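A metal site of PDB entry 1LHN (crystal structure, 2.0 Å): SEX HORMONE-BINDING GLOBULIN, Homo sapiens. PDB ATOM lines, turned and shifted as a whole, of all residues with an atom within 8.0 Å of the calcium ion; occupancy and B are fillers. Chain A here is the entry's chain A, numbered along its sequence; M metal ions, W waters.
The side-chain carboxylate (OE2) of Glu 52 sits at hydrogen-bond distance from the backbone NH (N) of Val 158.
OG1 of Thr 48 sits at hydrogen-bond distance from N of Asp 50 (2.9 Å).
The side-chain carboxylate (OD2) of Asp 50 sits close to the backbone NH (N) of Asp 162, at 2.8 Å.
Within 4 Å of the calcium ion: Asp 50, Glu 52 and Ala 160.
Water W3 binds the calcium ion (2.2 Å).
The side-chain carboxylate (OD2) of Asp 50 is bound to the calcium ion (2.2 Å).
The calcium ion is bound by O of Ala 160 (2.3 Å).
The backbone carbonyl oxygen (O) of Glu 52 is bound to the calcium ion, at 2.3 Å.
Water W1 is bound to the calcium ion, 2.4 Å away.
OD1 of Asp 50 is bound to the calcium ion, 2.5 Å away.
The calcium ion is bound by water W2 (2.5 Å).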
ATOM      1  N   SER A  19     -17.993  29.926  -1.754  1.00  0.00           N
ATOM      2  CA  SER A  19     -18.072  28.698  -0.973  1.00  0.00           C
ATOM      3  C   SER A  19     -16.882  28.635  -0.042  1.00  0.00           C
ATOM      4  O   SER A  19     -15.830  29.175  -0.347  1.00  0.00           O
ATOM      5  CB  SER A  19     -18.083  27.456  -1.876  1.00  0.00           C
ATOM      6  OG  SER A  19     -16.779  27.086  -2.273  1.00  0.00           O
ATOM      7  N   GLY A  23     -18.112  23.493   1.009  1.00  0.00           N
ATOM      8  CA  GLY A  23     -19.240  24.054   0.275  1.00  0.00           C
ATOM      9  C   GLY A  23     -20.505  23.225   0.449  1.00  0.00           C
ATOM     10  O   GLY A  23     -21.088  22.761  -0.529  1.00  0.00           O
ATOM     11  N   THR A  48     -16.098  32.499 -12.407  1.00  0.00           N
ATOM     12  CA  THR A  48     -15.853  31.130 -11.992  1.00  0.00           C
ATOM     13  C   THR A  48     -15.426  30.209 -13.140  1.00  0.00           C
ATOM     14  O   THR A  48     -15.653  30.521 -14.310  1.00  0.00           O
ATOM     15  CB  THR A  48     -17.124  30.530 -11.367  1.00  0.00           C
ATOM     16  OG1 THR A  48     -16.863  29.206 -10.891  1.00  0.00           O
ATOM     17  CG2 THR A  48     -18.254  30.481 -12.410  1.00  0.00           C
ATOM     18  N   TRP A  49     -14.807  29.079 -12.779  1.00  0.00           N
ATOM     19  CA  TRP A  49     -14.394  28.065 -13.735  1.00  0.00           C
ATOM     20  C   TRP A  49     -15.203  26.797 -13.433  1.00  0.00           C
ATOM     21  O   TRP A  49     -15.051  25.786 -14.111  1.00  0.00           O
ATOM     22  CB  TRP A  49     -12.892  27.707 -13.600  1.00  0.00           C
ATOM     23  CG  TRP A  49     -11.946  28.818 -13.982  1.00  0.00           C
ATOM     24  CD1 TRP A  49     -11.293  29.672 -13.128  1.00  0.00           C
ATOM     25  CD2 TRP A  49     -11.583  29.220 -15.304  1.00  0.00           C
ATOM     26  NE1 TRP A  49     -10.558  30.589 -13.849  1.00  0.00           N
ATOM     27  CE2 TRP A  49     -10.731  30.341 -15.184  1.00  0.00           C
ATOM     28  CE3 TRP A  49     -11.920  28.766 -16.586  1.00  0.00           C
ATOM     29  CZ2 TRP A  49     -10.195  31.005 -16.300  1.00  0.00           C
ATOM     30  CZ3 TRP A  49     -11.382  29.416 -17.690  1.00  0.00           C
ATOM     31  CH2 TRP A  49     -10.528  30.528 -17.536  1.00  0.00           C
ATOM     32  N   ASP A  50     -16.048  26.869 -12.403  1.00  0.00           N
ATOM     33  CA  ASP A  50     -16.857  25.745 -11.933  1.00  0.00           C
ATOM     34  C   ASP A  50     -18.134  25.620 -12.764  1.00  0.00           C
ATOM     35  O   ASP A  50     -18.920  26.566 -12.839  1.00  0.00           O
ATOM     36  CB  ASP A  50     -17.241  26.001 -10.469  1.00  0.00           C
ATOM     37  CG  ASP A  50     -17.732  24.761  -9.743  1.00  0.00           C
ATOM     38  OD1 ASP A  50     -18.132  23.762 -10.381  1.00  0.00           O
ATOM     39  OD2 ASP A  50     -17.726  24.805  -8.496  1.00  0.00           O
ATOM     40  N   PRO A  51     -18.353  24.449 -13.392  1.00  0.00           N
ATOM     41  CA  PRO A  51     -19.569  24.311 -14.205  1.00  0.00           C
ATOM     42  C   PRO A  51     -20.877  23.997 -13.459  1.00  0.00           C
ATOM     43  O   PRO A  51     -21.957  24.049 -14.064  1.00  0.00           O
ATOM     44  CB  PRO A  51     -19.188  23.188 -15.185  1.00  0.00           C
ATOM     45  CG  PRO A  51     -18.325  22.268 -14.326  1.00  0.00           C
ATOM     46  CD  PRO A  51     -17.435  23.302 -13.600  1.00  0.00           C
ATOM     47  N   GLU A  52     -20.799  23.658 -12.174  1.00  0.00           N
ATOM     48  CA  GLU A  52     -21.996  23.296 -11.407  1.00  0.00           C
ATOM     49  C   GLU A  52     -21.994  23.815  -9.980  1.00  0.00           C
ATOM     50  O   GLU A  52     -20.988  23.723  -9.301  1.00  0.00           O
ATOM     51  CB  GLU A  52     -22.138  21.779 -11.368  1.00  0.00           C
ATOM     52  CG  GLU A  52     -23.399  21.274 -10.665  1.00  0.00           C
ATOM     53  CD  GLU A  52     -23.639  19.786 -10.839  1.00  0.00           C
ATOM     54  OE1 GLU A  52     -23.603  19.296 -11.989  1.00  0.00           O
ATOM     55  OE2 GLU A  52     -23.894  19.112  -9.820  1.00  0.00           O
ATOM     56  N   GLY A  53     -23.130  24.339  -9.519  1.00  0.00           N
ATOM     57  CA  GLY A  53     -23.223  24.825  -8.160  1.00  0.00           C
ATOM     58  C   GLY A  53     -24.327  25.849  -7.955  1.00  0.00           C
ATOM     59  O   GLY A  53     -24.926  26.347  -8.907  1.00  0.00           O
ATOM     60  N   VAL A  54     -24.586  26.168  -6.688  1.00  0.00           N
ATOM     61  CA  VAL A  54     -25.613  27.140  -6.341  1.00  0.00           C
ATOM     62  C   VAL A  54     -25.037  28.554  -6.240  1.00  0.00           C
ATOM     63  O   VAL A  54     -24.079  28.793  -5.494  1.00  0.00           O
ATOM     64  CB  VAL A  54     -26.251  26.812  -4.976  1.00  0.00           C
ATOM     65  CG1 VAL A  54     -27.270  27.914  -4.600  1.00  0.00           C
ATOM     66  CG2 VAL A  54     -26.886  25.416  -4.988  1.00  0.00           C
ATOM     67  N   LEU A  71     -25.642  27.016 -11.565  1.00  0.00           N
ATOM     68  CA  LEU A  71     -25.044  26.673 -12.836  1.00  0.00           C
ATOM     69  C   LEU A  71     -25.084  25.152 -12.989  1.00  0.00           C
ATOM     70  O   LEU A  71     -24.942  24.414 -12.024  1.00  0.00           O
ATOM     71  CB  LEU A  71     -23.564  27.124 -12.900  1.00  0.00           C
ATOM     72  CG  LEU A  71     -23.221  28.621 -12.883  1.00  0.00           C
ATOM     73  CD1 LEU A  71     -21.685  28.750 -12.994  1.00  0.00           C
ATOM     74  CD2 LEU A  71     -23.943  29.394 -14.043  1.00  0.00           C
ATOM     75  N   LEU A 157     -28.138  18.701  -7.707  1.00  0.00           N
ATOM     76  CA  LEU A 157     -26.854  19.060  -8.291  1.00  0.00           C
ATOM     77  C   LEU A 157     -25.958  19.201  -7.052  1.00  0.00           C
ATOM     78  O   LEU A 157     -26.464  19.164  -5.926  1.00  0.00           O
ATOM     79  CB  LEU A 157     -26.912  20.381  -9.089  1.00  0.00           C
ATOM     80  CG  LEU A 157     -27.553  21.656  -8.525  1.00  0.00           C
ATOM     81  CD1 LEU A 157     -27.003  21.987  -7.123  1.00  0.00           C
ATOM     82  CD2 LEU A 157     -27.267  22.809  -9.486  1.00  0.00           C
ATOM     83  N   VAL A 158     -24.647  19.328  -7.252  1.00  0.00           N
ATOM     84  CA  VAL A 158     -23.730  19.487  -6.124  1.00  0.00           C
ATOM     85  C   VAL A 158     -23.633  21.000  -5.937  1.00  0.00           C
ATOM     86  O   VAL A 158     -23.094  21.713  -6.788  1.00  0.00           O
ATOM     87  CB  VAL A 158     -22.352  18.863  -6.423  1.00  0.00           C
ATOM     88  CG1 VAL A 158     -21.429  19.036  -5.215  1.00  0.00           C
ATOM     89  CG2 VAL A 158     -22.520  17.376  -6.768  1.00  0.00           C
ATOM     90  N   PRO A 159     -24.147  21.509  -4.810  1.00  0.00           N
ATOM     91  CA  PRO A 159     -24.167  22.941  -4.470  1.00  0.00           C
ATOM     92  C   PRO A 159     -22.889  23.757  -4.459  1.00  0.00           C
ATOM     93  O   PRO A 159     -22.903  24.919  -4.824  1.00  0.00           O
ATOM     94  CB  PRO A 159     -24.920  22.974  -3.126  1.00  0.00           C
ATOM     95  CG  PRO A 159     -24.570  21.646  -2.505  1.00  0.00           C
ATOM     96  CD  PRO A 159     -24.620  20.676  -3.676  1.00  0.00           C
ATOM     97  N   ALA A 160     -21.766  23.146  -4.073  1.00  0.00           N
ATOM     98  CA  ALA A 160     -20.516  23.882  -4.017  1.00  0.00           C
ATOM     99  C   ALA A 160     -20.158  24.592  -5.327  1.00  0.00           C
ATOM    100  O   ALA A 160     -20.009  23.973  -6.371  1.00  0.00           O
ATOM    101  CB  ALA A 160     -19.355  22.941  -3.594  1.00  0.00           C
ATOM    102  N   LEU A 161     -20.064  25.912  -5.257  1.00  0.00           N
ATOM    103  CA  LEU A 161     -19.682  26.663  -6.438  1.00  0.00           C
ATOM    104  C   LEU A 161     -18.393  27.427  -6.143  1.00  0.00           C
ATOM    105  O   LEU A 161     -18.382  28.373  -5.345  1.00  0.00           O
ATOM    106  CB  LEU A 161     -20.782  27.632  -6.867  1.00  0.00           C
ATOM    107  CG  LEU A 161     -20.431  28.360  -8.172  1.00  0.00           C
ATOM    108  CD1 LEU A 161     -20.420  27.355  -9.324  1.00  0.00           C
ATOM    109  CD2 LEU A 161     -21.438  29.460  -8.448  1.00  0.00           C
ATOM    110  N   ASP A 162     -17.309  27.001  -6.788  1.00  0.00           N
ATOM    111  CA  ASP A 162     -16.008  27.625  -6.621  1.00  0.00           C
ATOM    112  C   ASP A 162     -15.929  28.866  -7.488  1.00  0.00           C
ATOM    113  O   ASP A 162     -15.462  28.822  -8.623  1.00  0.00           O
ATOM    114  CB  ASP A 162     -14.911  26.636  -7.040  1.00  0.00           C
ATOM    115  CG  ASP A 162     -13.527  27.070  -6.588  1.00  0.00           C
ATOM    116  OD1 ASP A 162     -13.311  28.289  -6.372  1.00  0.00           O
ATOM    117  OD2 ASP A 162     -12.647  26.197  -6.469  1.00  0.00           O
ATOM    118  N   GLY A 163     -16.400  29.987  -6.955  1.00  0.00           N
ATOM    119  CA  GLY A 163     -16.374  31.201  -7.725  1.00  0.00           C
ATOM    120  C   GLY A 163     -16.355  32.443  -6.850  1.00  0.00           C
ATOM    121  O   GLY A 163     -16.401  32.356  -5.616  1.00  0.00           O
HETATM  122 CA    CA M   1     -19.063  23.041  -8.215  1.00  0.00          CA
HETATM  123  O   HOH W   1     -17.363  21.906  -6.972  1.00  0.00           O
HETATM  124  O   HOH W   2     -18.546  21.216  -9.879  1.00  0.00           O
HETATM  125  O   HOH W   3     -20.261  21.320  -7.558  1.00  0.00           O
